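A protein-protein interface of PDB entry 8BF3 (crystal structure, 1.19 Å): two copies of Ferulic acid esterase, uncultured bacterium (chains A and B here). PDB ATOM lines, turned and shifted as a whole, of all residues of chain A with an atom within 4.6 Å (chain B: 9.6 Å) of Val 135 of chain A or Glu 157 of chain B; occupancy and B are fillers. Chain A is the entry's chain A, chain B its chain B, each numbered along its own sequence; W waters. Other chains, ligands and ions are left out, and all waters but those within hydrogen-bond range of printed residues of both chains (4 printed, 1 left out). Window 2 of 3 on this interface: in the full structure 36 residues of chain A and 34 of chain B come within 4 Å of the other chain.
The backbone NH (N) of Gly 158 of chain B is in hydrogen-bond range of the side-chain amide oxygen (OD1) of Asn 256 of chain A, 3.0 Å away.
O of Val 132 of chain B sits at hydrogen-bond distance from N of Lys 134 of chain A.
The backbone carbonyl oxygen (O) of Thr 133 of chain B is in hydrogen-bond range of the backbone NH (N) of Val 150 of chain B, at 2.8 Å.
The backbone NH (N) of Val 150 of chain A sits at hydrogen-bond distance from the backbone carbonyl oxygen (O) of Thr 133 of chain A.
The backbone carbonyl oxygen (O) of Thr 131 of chain B lies within hydrogen-bond range of the backbone NH (N) of Thr 152 of chain B.
ND2 of Asn 256 of chain A sits at hydrogen-bond distance from O of Phe 252 of chain A.
The side-chain hydroxyl (OG1) of Thr 131 of chain B sits at hydrogen-bond distance from the side-chain carboxylate (OE2) of Glu 157 of chain B, at 2.6 Å.
O of Val 135 of chain A lies within hydrogen-bond range of N of Met 148 of chain A, at 2.9 Å.
Thr 131 of chain B touches Thr 133 of chain A (CG2 to CG2, 3.3 Å).
Thr 133 of chain A touches Val 132 of chain B (CA to O, 3.7 Å).
Thr 133 of chain A touches Thr 133 of chain B.
Lys 134 of chain A touches Lys 134 of chain B.
OG1 of Thr 131 of chain B touches CG2 of Val 135 of chain A, at 3.5 Å.
OE2 of Glu 157 of chain B touches CG2 of Val 135 of chain A, at 3.7 Å.
Trp 136 of chain A touches His 123 of chain B.
His 129 of chain B touches Trp 136 of chain A (CB to NE1, 3.4 Å).
CD1 of Trp 136 of chain A touches O of Gly 130 of chain B, 3.96 Å away.
Asn 256 of chain A touches Glu 157 of chain B.
Printed residues of chain B within 4 Å of Thr 133 of chain A: Thr 131 (3.3 Å), Val 132 (3.7 Å) and Thr 133 (3.6 Å).
Val 135 of chain A touches just these residues of chain B: Thr 131 (3.5 Å) and Glu 157 (3.7 Å).
Of the printed residues of chain B, Trp 136 of chain A touches His 123 (3.5 Å), His 129 (3.4 Å) and Gly 130 (3.96 Å).
Of the printed residues of chain B, Asn 256 of chain A touches Glu 157 (3.7 Å) and Gly 158 (3.0 Å).
Of the printed residues of chain A, Lys 134 of chain B touches Lys 134.
Val 150 of chain B touches none of the printed residues of chain A.
Glu 157 of chain B touches two residues of chain A.
Of the printed residues of chain A, Gly 158 of chain B touches Asn 256.
Arg 258 of chain B touches none of the printed residues of chain A.
The nearest printed residue of chain A that does not touch Val 132 of chain B is Val 135 of chain A (5.2 Å).
Of the 23 printed residues of chain B, 9 touch a printed residue of chain A.
Hydrophobic or aromatic side chains of chain B that line the printed part of chain A: His 123 and His 129.
Along chain A the printed residues that touch a printed residue of chain B span positions 133 to 256.
Among the printed residues, 13 pairs touch across the chains.
Thr 133 of chain B touches its own counterpart, Thr 133 of chain A.
Lys 134 of chain B touches its own counterpart, Lys 134 of chain A.
Water W4 bridges O of Trp 136 of chain A (2.7 Å) and OE1 of Glu 157 of chain B (2.9 Å).
Water W2 lies within hydrogen-bond range of the side-chain hydroxyl (OG1) of Thr 131 of chain B (2.7 Å), the backbone carbonyl oxygen (O) of His 129 of chain B (2.8 Å) and the backbone NH (N) of Trp 136 of chain A (2.9 Å).
Water W1 lies within hydrogen-bond range of O of Gly 130 of chain B (2.8 Å), O of Lys 134 of chain A (2.8 Å) and NE1 of Trp 136 of chain A (3.2 Å).
Water W3 bridges NZ of Lys 134 of chain B (2.8 Å) and NZ of Lys 134 of chain A (2.8 Å).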
ATOM      1  N   THR A 133      -8.468   2.593  -1.693  1.00  0.00           N
ATOM      2  CA  THR A 133      -7.139   2.255  -1.211  1.00  0.00           C
ATOM      3  C   THR A 133      -6.953   2.819   0.184  1.00  0.00           C
ATOM      4  O   THR A 133      -7.170   4.011   0.400  1.00  0.00           O
ATOM      5  CB  THR A 133      -6.088   2.851  -2.156  1.00  0.00           C
ATOM      6  OG1 THR A 133      -6.265   2.312  -3.474  1.00  0.00           O
ATOM      7  CG2 THR A 133      -4.689   2.523  -1.701  1.00  0.00           C
ATOM      8  N   LYS A 134      -6.566   1.960   1.120  1.00  0.00           N
ATOM      9  CA  LYS A 134      -6.281   2.351   2.498  1.00  0.00           C
ATOM     10  C   LYS A 134      -4.764   2.414   2.613  1.00  0.00           C
ATOM     11  O   LYS A 134      -4.102   1.375   2.712  1.00  0.00           O
ATOM     12  CB  LYS A 134      -6.865   1.334   3.469  1.00  0.00           C
ATOM     13  CG  LYS A 134      -8.339   1.023   3.278  1.00  0.00           C
ATOM     14  CD  LYS A 134      -8.836   0.186   4.439  1.00  0.00           C
ATOM     15  CE  LYS A 134     -10.244  -0.278   4.282  1.00  0.00           C
ATOM     16  NZ  LYS A 134     -10.781  -0.771   5.594  1.00  0.00           N
ATOM     17  N   VAL A 135      -4.223   3.626   2.547  1.00  0.00           N
ATOM     18  CA  VAL A 135      -2.798   3.843   2.345  1.00  0.00           C
ATOM     19  C   VAL A 135      -2.231   4.660   3.499  1.00  0.00           C
ATOM     20  O   VAL A 135      -2.860   5.614   3.980  1.00  0.00           O
ATOM     21  CB  VAL A 135      -2.523   4.490   0.967  1.00  0.00           C
ATOM     22  CG1 VAL A 135      -3.299   5.775   0.794  1.00  0.00           C
ATOM     23  CG2 VAL A 135      -1.026   4.717   0.755  1.00  0.00           C
ATOM     24  N   TRP A 136      -1.019   4.297   3.916  1.00  0.00           N
ATOM     25  CA  TRP A 136      -0.287   4.996   4.958  1.00  0.00           C
ATOM     26  C   TRP A 136       0.753   5.927   4.350  1.00  0.00           C
ATOM     27  O   TRP A 136       1.308   5.663   3.280  1.00  0.00           O
ATOM     28  CB  TRP A 136       0.393   3.988   5.881  1.00  0.00           C
ATOM     29  CG  TRP A 136      -0.583   3.190   6.673  1.00  0.00           C
ATOM     30  CD1 TRP A 136      -1.301   2.109   6.247  1.00  0.00           C
ATOM     31  CD2 TRP A 136      -0.970   3.428   8.034  1.00  0.00           C
ATOM     32  NE1 TRP A 136      -2.109   1.655   7.271  1.00  0.00           N
ATOM     33  CE2 TRP A 136      -1.913   2.442   8.379  1.00  0.00           C
ATOM     34  CE3 TRP A 136      -0.595   4.371   8.997  1.00  0.00           C
ATOM     35  CZ2 TRP A 136      -2.500   2.380   9.642  1.00  0.00           C
ATOM     36  CZ3 TRP A 136      -1.174   4.306  10.245  1.00  0.00           C
ATOM     37  CH2 TRP A 136      -2.119   3.323  10.555  1.00  0.00           C
ATOM     38  N   TYR A 137       1.026   7.019   5.052  1.00  0.00           N
ATOM     39  CA  TYR A 137       1.973   8.014   4.567  1.00  0.00           C
ATOM     40  C   TYR A 137       2.687   8.617   5.764  1.00  0.00           C
ATOM     41  O   TYR A 137       2.137   8.705   6.862  1.00  0.00           O
ATOM     42  CB  TYR A 137       1.261   9.098   3.734  1.00  0.00           C
ATOM     43  CG  TYR A 137       0.195   9.839   4.507  1.00  0.00           C
ATOM     44  CD1 TYR A 137      -1.073   9.298   4.680  1.00  0.00           C
ATOM     45  CD2 TYR A 137       0.454  11.076   5.068  1.00  0.00           C
ATOM     46  CE1 TYR A 137      -2.046   9.969   5.399  1.00  0.00           C
ATOM     47  CE2 TYR A 137      -0.507  11.738   5.801  1.00  0.00           C
ATOM     48  CZ  TYR A 137      -1.757  11.183   5.964  1.00  0.00           C
ATOM     49  OH  TYR A 137      -2.730  11.828   6.695  1.00  0.00           O
ATOM     50  N   ARG A 146       0.386   7.998   9.155  1.00  0.00           N
ATOM     51  CA  ARG A 146      -1.062   8.037   9.283  1.00  0.00           C
ATOM     52  C   ARG A 146      -1.710   7.370   8.081  1.00  0.00           C
ATOM     53  O   ARG A 146      -1.081   7.186   7.039  1.00  0.00           O
ATOM     54  CB  ARG A 146      -1.524   9.494   9.381  1.00  0.00           C
ATOM     55  CG  ARG A 146      -0.764  10.278  10.432  1.00  0.00           C
ATOM     56  CD  ARG A 146      -1.305  11.694  10.656  1.00  0.00           C
ATOM     57  NE  ARG A 146      -2.564  11.678  11.400  1.00  0.00           N
ATOM     58  CZ  ARG A 146      -3.755  12.036  10.932  1.00  0.00           C
ATOM     59  NH1 ARG A 146      -3.923  12.465   9.695  1.00  0.00           N
ATOM     60  NH2 ARG A 146      -4.800  11.995  11.743  1.00  0.00           N
ATOM     61  N   ARG A 147      -2.983   7.018   8.237  1.00  0.00           N
ATOM     62  CA  ARG A 147      -3.731   6.307   7.216  1.00  0.00           C
ATOM     63  C   ARG A 147      -4.805   7.209   6.632  1.00  0.00           C
ATOM     64  O   ARG A 147      -5.467   7.958   7.354  1.00  0.00           O
ATOM     65  CB  ARG A 147      -4.385   5.046   7.784  1.00  0.00           C
ATOM     66  CG  ARG A 147      -4.833   4.077   6.703  1.00  0.00           C
ATOM     67  CD  ARG A 147      -5.433   2.786   7.249  1.00  0.00           C
ATOM     68  NE  ARG A 147      -6.716   3.040   7.890  1.00  0.00           N
ATOM     69  CZ  ARG A 147      -7.577   2.100   8.243  1.00  0.00           C
ATOM     70  NH1 ARG A 147      -7.371   0.824   7.950  1.00  0.00           N
ATOM     71  NH2 ARG A 147      -8.673   2.449   8.905  1.00  0.00           N
ATOM     72  N   MET A 148      -4.993   7.109   5.321  1.00  0.00           N
ATOM     73  CA  MET A 148      -6.100   7.761   4.636  1.00  0.00           C
ATOM     74  C   MET A 148      -6.724   6.775   3.656  1.00  0.00           C
ATOM     75  O   MET A 148      -6.131   5.745   3.312  1.00  0.00           O
ATOM     76  CB  MET A 148      -5.669   9.029   3.882  1.00  0.00           C
ATOM     77  CG  MET A 148      -4.566   8.826   2.866  1.00  0.00           C
ATOM     78  SD  MET A 148      -4.081  10.405   2.169  1.00  0.00           S
ATOM     79  CE  MET A 148      -2.533   9.958   1.392  1.00  0.00           C
ATOM     80  N   VAL A 150      -8.262   6.516  -0.216  1.00  0.00           N
ATOM     81  CA  VAL A 150      -8.240   7.192  -1.506  1.00  0.00           C
ATOM     82  C   VAL A 150      -9.134   6.416  -2.461  1.00  0.00           C
ATOM     83  O   VAL A 150      -8.918   5.221  -2.685  1.00  0.00           O
ATOM     84  CB  VAL A 150      -6.824   7.321  -2.079  1.00  0.00           C
ATOM     85  CG1 VAL A 150      -6.863   8.061  -3.405  1.00  0.00           C
ATOM     86  CG2 VAL A 150      -5.921   8.044  -1.104  1.00  0.00           C
ATOM     87  N   PHE A 252       2.004  13.774  -1.201  1.00  0.00           N
ATOM     88  CA  PHE A 252       1.986  12.319  -1.299  1.00  0.00           C
ATOM     89  C   PHE A 252       1.012  11.874  -2.382  1.00  0.00           C
ATOM     90  O   PHE A 252       1.315  10.981  -3.180  1.00  0.00           O
ATOM     91  CB  PHE A 252       1.601  11.722   0.060  1.00  0.00           C
ATOM     92  CG  PHE A 252       1.572  10.214   0.079  1.00  0.00           C
ATOM     93  CD1 PHE A 252       0.444   9.515  -0.326  1.00  0.00           C
ATOM     94  CD2 PHE A 252       2.662   9.494   0.513  1.00  0.00           C
ATOM     95  CE1 PHE A 252       0.418   8.129  -0.304  1.00  0.00           C
ATOM     96  CE2 PHE A 252       2.645   8.103   0.522  1.00  0.00           C
ATOM     97  CZ  PHE A 252       1.512   7.430   0.123  1.00  0.00           C
ATOM     98  N   ASN A 256       2.161   9.819  -5.775  1.00  0.00           N
ATOM     99  CA  ASN A 256       1.849   8.397  -5.799  1.00  0.00           C
ATOM    100  C   ASN A 256       0.571   8.033  -6.528  1.00  0.00           C
ATOM    101  O   ASN A 256       0.288   6.836  -6.688  1.00  0.00           O
ATOM    102  CB  ASN A 256       1.830   7.867  -4.362  1.00  0.00           C
ATOM    103  CG  ASN A 256       3.195   7.906  -3.749  1.00  0.00           C
ATOM    104  OD1 ASN A 256       4.115   7.298  -4.266  1.00  0.00           O
ATOM    105  ND2 ASN A 256       3.349   8.646  -2.684  1.00  0.00           N
ATOM    106  N   HIS B 123      -2.089  -4.582  15.569  1.00  0.00           N
ATOM    107  CA  HIS B 123      -1.709  -3.424  14.785  1.00  0.00           C
ATOM    108  C   HIS B 123      -0.838  -2.541  15.665  1.00  0.00           C
ATOM    109  O   HIS B 123      -1.322  -1.957  16.636  1.00  0.00           O
ATOM    110  CB  HIS B 123      -2.936  -2.649  14.331  1.00  0.00           C
ATOM    111  CG  HIS B 123      -2.592  -1.552  13.389  1.00  0.00           C
ATOM    112  ND1 HIS B 123      -2.614  -1.720  12.022  1.00  0.00           N
ATOM    113  CD2 HIS B 123      -2.124  -0.306  13.616  1.00  0.00           C
ATOM    114  CE1 HIS B 123      -2.223  -0.597  11.448  1.00  0.00           C
ATOM    115  NE2 HIS B 123      -1.916   0.274  12.393  1.00  0.00           N
ATOM    116  N   PRO B 128       5.931   0.081  10.185  1.00  0.00           N
ATOM    117  CA  PRO B 128       5.428   0.579   8.896  1.00  0.00           C
ATOM    118  C   PRO B 128       4.307  -0.307   8.374  1.00  0.00           C
ATOM    119  O   PRO B 128       4.377  -1.533   8.458  1.00  0.00           O
ATOM    120  CB  PRO B 128       6.665   0.511   7.987  1.00  0.00           C
ATOM    121  CG  PRO B 128       7.827   0.514   8.886  1.00  0.00           C
ATOM    122  CD  PRO B 128       7.366  -0.242  10.105  1.00  0.00           C
ATOM    123  N   HIS B 129       3.282   0.311   7.800  1.00  0.00           N
ATOM    124  CA  HIS B 129       2.085  -0.426   7.407  1.00  0.00           C
ATOM    125  C   HIS B 129       1.881  -0.477   5.901  1.00  0.00           C
ATOM    126  O   HIS B 129       1.942   0.553   5.221  1.00  0.00           O
ATOM    127  CB  HIS B 129       0.842   0.169   8.069  1.00  0.00           C
ATOM    128  CG  HIS B 129       0.927   0.152   9.555  1.00  0.00           C
ATOM    129  ND1 HIS B 129       1.119  -1.013  10.261  1.00  0.00           N
ATOM    130  CD2 HIS B 129       0.898   1.149  10.468  1.00  0.00           C
ATOM    131  CE1 HIS B 129       1.191  -0.735  11.551  1.00  0.00           C
ATOM    132  NE2 HIS B 129       1.065   0.571  11.703  1.00  0.00           N
ATOM    133  N   GLY B 130       1.583  -1.672   5.411  1.00  0.00           N
ATOM    134  CA  GLY B 130       1.274  -1.850   4.011  1.00  0.00           C
ATOM    135  C   GLY B 130      -0.134  -1.409   3.652  1.00  0.00           C
ATOM    136  O   GLY B 130      -1.053  -1.417   4.464  1.00  0.00           O
ATOM    137  N   THR B 131      -0.296  -1.029   2.390  1.00  0.00           N
ATOM    138  CA  THR B 131      -1.582  -0.619   1.854  1.00  0.00           C
ATOM    139  C   THR B 131      -2.477  -1.821   1.605  1.00  0.00           C
ATOM    140  O   THR B 131      -2.013  -2.889   1.197  1.00  0.00           O
ATOM    141  CB  THR B 131      -1.324   0.121   0.539  1.00  0.00           C
ATOM    142  OG1 THR B 131      -0.570   1.297   0.833  1.00  0.00           O
ATOM    143  CG2 THR B 131      -2.592   0.507  -0.181  1.00  0.00           C
ATOM    144  N   VAL B 132      -3.772  -1.626   1.841  1.00  0.00           N
ATOM    145  CA  VAL B 132      -4.801  -2.573   1.435  1.00  0.00           C
ATOM    146  C   VAL B 132      -5.669  -1.878   0.401  1.00  0.00           C
ATOM    147  O   VAL B 132      -6.264  -0.832   0.687  1.00  0.00           O
ATOM    148  CB  VAL B 132      -5.639  -3.085   2.616  1.00  0.00           C
ATOM    149  CG1 VAL B 132      -6.726  -4.008   2.105  1.00  0.00           C
ATOM    150  CG2 VAL B 132      -4.739  -3.779   3.643  1.00  0.00           C
ATOM    151  N   THR B 133      -5.720  -2.451  -0.795  1.00  0.00           N
ATOM    152  CA  THR B 133      -6.445  -1.901  -1.929  1.00  0.00           C
ATOM    153  C   THR B 133      -7.616  -2.809  -2.266  1.00  0.00           C
ATOM    154  O   THR B 133      -7.434  -4.017  -2.447  1.00  0.00           O
ATOM    155  CB  THR B 133      -5.492  -1.807  -3.125  1.00  0.00           C
ATOM    156  OG1 THR B 133      -4.367  -0.995  -2.780  1.00  0.00           O
ATOM    157  CG2 THR B 133      -6.180  -1.204  -4.305  1.00  0.00           C
ATOM    158  N   LYS B 134      -8.803  -2.228  -2.337  1.00  0.00           N
ATOM    159  CA  LYS B 134     -10.021  -2.940  -2.714  1.00  0.00           C
ATOM    160  C   LYS B 134     -10.291  -2.573  -4.168  1.00  0.00           C
ATOM    161  O   LYS B 134     -10.785  -1.479  -4.464  1.00  0.00           O
ATOM    162  CB  LYS B 134     -11.190  -2.548  -1.818  1.00  0.00           C
ATOM    163  CG  LYS B 134     -10.925  -2.649  -0.325  1.00  0.00           C
ATOM    164  CD  LYS B 134     -12.232  -2.498   0.448  1.00  0.00           C
ATOM    165  CE  LYS B 134     -12.045  -2.391   1.930  1.00  0.00           C
ATOM    166  NZ  LYS B 134     -13.366  -2.552   2.633  1.00  0.00           N
ATOM    167  N   VAL B 150      -5.941  -6.389  -2.256  1.00  0.00           N
ATOM    168  CA  VAL B 150      -4.512  -6.558  -2.482  1.00  0.00           C
ATOM    169  C   VAL B 150      -3.743  -5.817  -1.399  1.00  0.00           C
ATOM    170  O   VAL B 150      -3.929  -4.604  -1.205  1.00  0.00           O
ATOM    171  CB  VAL B 150      -4.082  -6.061  -3.867  1.00  0.00           C
ATOM    172  CG1 VAL B 150      -2.599  -6.308  -4.074  1.00  0.00           C
ATOM    173  CG2 VAL B 150      -4.905  -6.741  -4.943  1.00  0.00           C
ATOM    174  N   TYR B 151      -2.885  -6.546  -0.701  1.00  0.00           N
ATOM    175  CA  TYR B 151      -1.939  -5.977   0.247  1.00  0.00           C
ATOM    176  C   TYR B 151      -0.617  -5.750  -0.472  1.00  0.00           C
ATOM    177  O   TYR B 151      -0.105  -6.655  -1.133  1.00  0.00           O
ATOM    178  CB  TYR B 151      -1.729  -6.952   1.403  1.00  0.00           C
ATOM    179  CG  TYR B 151      -0.612  -6.584   2.351  1.00  0.00           C
ATOM    180  CD1 TYR B 151       0.685  -7.011   2.127  1.00  0.00           C
ATOM    181  CD2 TYR B 151      -0.855  -5.851   3.502  1.00  0.00           C
ATOM    182  CE1 TYR B 151       1.702  -6.699   2.997  1.00  0.00           C
ATOM    183  CE2 TYR B 151       0.163  -5.530   4.380  1.00  0.00           C
ATOM    184  CZ  TYR B 151       1.441  -5.959   4.113  1.00  0.00           C
ATOM    185  OH  TYR B 151       2.464  -5.669   4.984  1.00  0.00           O
ATOM    186  N   THR B 152      -0.086  -4.537  -0.358  1.00  0.00           N
ATOM    187  CA  THR B 152       1.267  -4.263  -0.802  1.00  0.00           C
ATOM    188  C   THR B 152       2.120  -3.915   0.413  1.00  0.00           C
ATOM    189  O   THR B 152       1.616  -3.373   1.405  1.00  0.00           O
ATOM    190  CB  THR B 152       1.319  -3.126  -1.832  1.00  0.00           C
ATOM    191  OG1 THR B 152       0.560  -2.009  -1.357  1.00  0.00           O
ATOM    192  CG2 THR B 152       0.745  -3.570  -3.155  1.00  0.00           C
ATOM    193  N   PRO B 153       3.406  -4.235   0.379  1.00  0.00           N
ATOM    194  CA  PRO B 153       4.232  -4.065   1.570  1.00  0.00           C
ATOM    195  C   PRO B 153       4.481  -2.591   1.857  1.00  0.00           C
ATOM    196  O   PRO B 153       4.366  -1.722   0.990  1.00  0.00           O
ATOM    197  CB  PRO B 153       5.520  -4.812   1.211  1.00  0.00           C
ATOM    198  CG  PRO B 153       5.589  -4.735  -0.258  1.00  0.00           C
ATOM    199  CD  PRO B 153       4.163  -4.849  -0.727  1.00  0.00           C
ATOM    200  N   ALA B 154       4.830  -2.312   3.106  1.00  0.00           N
ATOM    201  CA  ALA B 154       5.154  -0.945   3.486  1.00  0.00           C
ATOM    202  C   ALA B 154       6.260  -0.407   2.597  1.00  0.00           C
ATOM    203  O   ALA B 154       7.215  -1.114   2.281  1.00  0.00           O
ATOM    204  CB  ALA B 154       5.600  -0.894   4.944  1.00  0.00           C
ATOM    205  N   GLY B 155       6.127   0.860   2.206  1.00  0.00           N
ATOM    206  CA  GLY B 155       7.087   1.487   1.325  1.00  0.00           C
ATOM    207  C   GLY B 155       6.915   1.180  -0.145  1.00  0.00           C
ATOM    208  O   GLY B 155       7.712   1.664  -0.960  1.00  0.00           O
ATOM    209  N   TYR B 156       5.917   0.379  -0.514  1.00  0.00           N
ATOM    210  CA  TYR B 156       5.628   0.147  -1.924  1.00  0.00           C
ATOM    211  C   TYR B 156       5.489   1.469  -2.653  1.00  0.00           C
ATOM    212  O   TYR B 156       6.081   1.677  -3.717  1.00  0.00           O
ATOM    213  CB  TYR B 156       4.332  -0.653  -2.031  1.00  0.00           C
ATOM    214  CG  TYR B 156       3.868  -0.965  -3.432  1.00  0.00           C
ATOM    215  CD1 TYR B 156       2.997  -0.119  -4.096  1.00  0.00           C
ATOM    216  CD2 TYR B 156       4.248  -2.141  -4.062  1.00  0.00           C
ATOM    217  CE1 TYR B 156       2.551  -0.419  -5.366  1.00  0.00           C
ATOM    218  CE2 TYR B 156       3.800  -2.448  -5.319  1.00  0.00           C
ATOM    219  CZ  TYR B 156       2.953  -1.590  -5.969  1.00  0.00           C
ATOM    220  OH  TYR B 156       2.511  -1.920  -7.222  1.00  0.00           O
ATOM    221  N   GLU B 157       4.707   2.376  -2.083  1.00  0.00           N
ATOM    222  CA  GLU B 157       4.501   3.685  -2.675  1.00  0.00           C
ATOM    223  C   GLU B 157       5.782   4.495  -2.599  1.00  0.00           C
ATOM    224  O   GLU B 157       6.430   4.567  -1.552  1.00  0.00           O
ATOM    225  CB  GLU B 157       3.382   4.408  -1.930  1.00  0.00           C
ATOM    226  CG  GLU B 157       1.979   3.817  -2.165  1.00  0.00           C
ATOM    227  CD  GLU B 157       1.610   2.640  -1.269  1.00  0.00           C
ATOM    228  OE1 GLU B 157       2.432   2.183  -0.435  1.00  0.00           O
ATOM    229  OE2 GLU B 157       0.471   2.153  -1.419  1.00  0.00           O
ATOM    230  N   GLY B 158       6.149   5.104  -3.710  1.00  0.00           N
ATOM    231  CA  GLY B 158       7.285   5.999  -3.725  1.00  0.00           C
ATOM    232  C   GLY B 158       8.590   5.347  -4.095  1.00  0.00           C
ATOM    233  O   GLY B 158       9.636   6.010  -4.048  1.00  0.00           O
ATOM    234  N   ASP B 159       8.565   4.078  -4.469  1.00  0.00           N
ATOM    235  CA  ASP B 159       9.757   3.334  -4.826  1.00  0.00           C
ATOM    236  C   ASP B 159       9.472   2.592  -6.123  1.00  0.00           C
ATOM    237  O   ASP B 159       8.337   2.561  -6.601  1.00  0.00           O
ATOM    238  CB  ASP B 159      10.126   2.377  -3.690  1.00  0.00           C
ATOM    239  CG  ASP B 159      11.443   1.682  -3.918  1.00  0.00           C
ATOM    240  OD1 ASP B 159      12.439   2.382  -4.199  1.00  0.00           O
ATOM    241  OD2 ASP B 159      11.485   0.439  -3.810  1.00  0.00           O
ATOM    242  N   THR B 160      10.522   2.010  -6.712  1.00  0.00           N
ATOM    243  CA  THR B 160      10.416   1.316  -7.988  1.00  0.00           C
ATOM    244  C   THR B 160      10.575  -0.190  -7.870  1.00  0.00           C
ATOM    245  O   THR B 160      10.409  -0.892  -8.871  1.00  0.00           O
ATOM    246  CB  THR B 160      11.501   1.823  -8.949  1.00  0.00           C
ATOM    247  OG1 THR B 160      12.776   1.698  -8.311  1.00  0.00           O
ATOM    248  CG2 THR B 160      11.249   3.268  -9.334  1.00  0.00           C
ATOM    249  N   GLN B 161      10.917  -0.697  -6.689  1.00  0.00           N
ATOM    250  CA  GLN B 161      11.165  -2.121  -6.506  1.00  0.00           C
ATOM    251  C   GLN B 161       9.941  -2.944  -6.885  1.00  0.00           C
ATOM    252  O   GLN B 161       8.801  -2.537  -6.654  1.00  0.00           O
ATOM    253  CB  GLN B 161      11.484  -2.338  -5.025  1.00  0.00           C
ATOM    254  CG  GLN B 161      11.932  -3.708  -4.639  1.00  0.00           C
ATOM    255  CD  GLN B 161      12.389  -3.759  -3.195  1.00  0.00           C
ATOM    256  OE1 GLN B 161      12.745  -2.731  -2.608  1.00  0.00           O
ATOM    257  NE2 GLN B 161      12.380  -4.951  -2.613  1.00  0.00           N
ATOM    258  N   TYR B 163       8.042  -6.869  -6.464  1.00  0.00           N
ATOM    259  CA  TYR B 163       7.825  -7.769  -5.340  1.00  0.00           C
ATOM    260  C   TYR B 163       7.203  -9.077  -5.798  1.00  0.00           C
ATOM    261  O   TYR B 163       6.364  -9.083  -6.705  1.00  0.00           O
ATOM    262  CB  TYR B 163       6.885  -7.120  -4.311  1.00  0.00           C
ATOM    263  CG  TYR B 163       7.514  -5.909  -3.680  1.00  0.00           C
ATOM    264  CD1 TYR B 163       8.431  -6.051  -2.655  1.00  0.00           C
ATOM    265  CD2 TYR B 163       7.221  -4.625  -4.124  1.00  0.00           C
ATOM    266  CE1 TYR B 163       9.030  -4.962  -2.075  1.00  0.00           C
ATOM    267  CE2 TYR B 163       7.831  -3.515  -3.552  1.00  0.00           C
ATOM    268  CZ  TYR B 163       8.736  -3.695  -2.525  1.00  0.00           C
ATOM    269  OH  TYR B 163       9.354  -2.622  -1.918  1.00  0.00           O
ATOM    270  N   PHE B 257       0.280  -3.935 -10.766  1.00  0.00           N
ATOM    271  CA  PHE B 257       1.144  -3.835  -9.604  1.00  0.00           C
ATOM    272  C   PHE B 257       2.565  -4.152 -10.036  1.00  0.00           C
ATOM    273  O   PHE B 257       2.790  -4.807 -11.055  1.00  0.00           O
ATOM    274  CB  PHE B 257       0.685  -4.792  -8.489  1.00  0.00           C
ATOM    275  CG  PHE B 257      -0.653  -4.426  -7.908  1.00  0.00           C
ATOM    276  CD1 PHE B 257      -1.824  -4.805  -8.538  1.00  0.00           C
ATOM    277  CD2 PHE B 257      -0.739  -3.663  -6.755  1.00  0.00           C
ATOM    278  CE1 PHE B 257      -3.049  -4.448  -8.031  1.00  0.00           C
ATOM    279  CE2 PHE B 257      -1.971  -3.309  -6.244  1.00  0.00           C
ATOM    280  CZ  PHE B 257      -3.120  -3.692  -6.888  1.00  0.00           C
ATOM    281  N   ARG B 258       3.524  -3.691  -9.233  1.00  0.00           N
ATOM    282  CA  ARG B 258       4.948  -3.899  -9.521  1.00  0.00           C
ATOM    283  C   ARG B 258       5.337  -5.292  -9.030  1.00  0.00           C
ATOM    284  O   ARG B 258       5.953  -5.470  -7.976  1.00  0.00           O
ATOM    285  CB  ARG B 258       5.793  -2.814  -8.867  1.00  0.00           C
ATOM    286  CG  ARG B 258       5.447  -1.413  -9.316  1.00  0.00           C
ATOM    287  CD  ARG B 258       6.584  -0.425  -9.061  1.00  0.00           C
ATOM    288  NE  ARG B 258       7.166  -0.556  -7.728  1.00  0.00           N
ATOM    289  CZ  ARG B 258       6.713   0.053  -6.639  1.00  0.00           C
ATOM    290  NH1 ARG B 258       5.684   0.890  -6.684  1.00  0.00           N
ATOM    291  NH2 ARG B 258       7.299  -0.196  -5.472  1.00  0.00           N
HETATM  292  O   HOH W   1      -3.427  -0.096   4.976  1.00  0.00           O
HETATM  293  O   HOH W   2       0.652   2.004   3.141  1.00  0.00           O
HETATM  294  O   HOH W   3     -13.211  -2.093   5.362  1.00  0.00           O
HETATM  295  O   HOH W   4       2.774   3.950   1.820  1.00  0.00           O
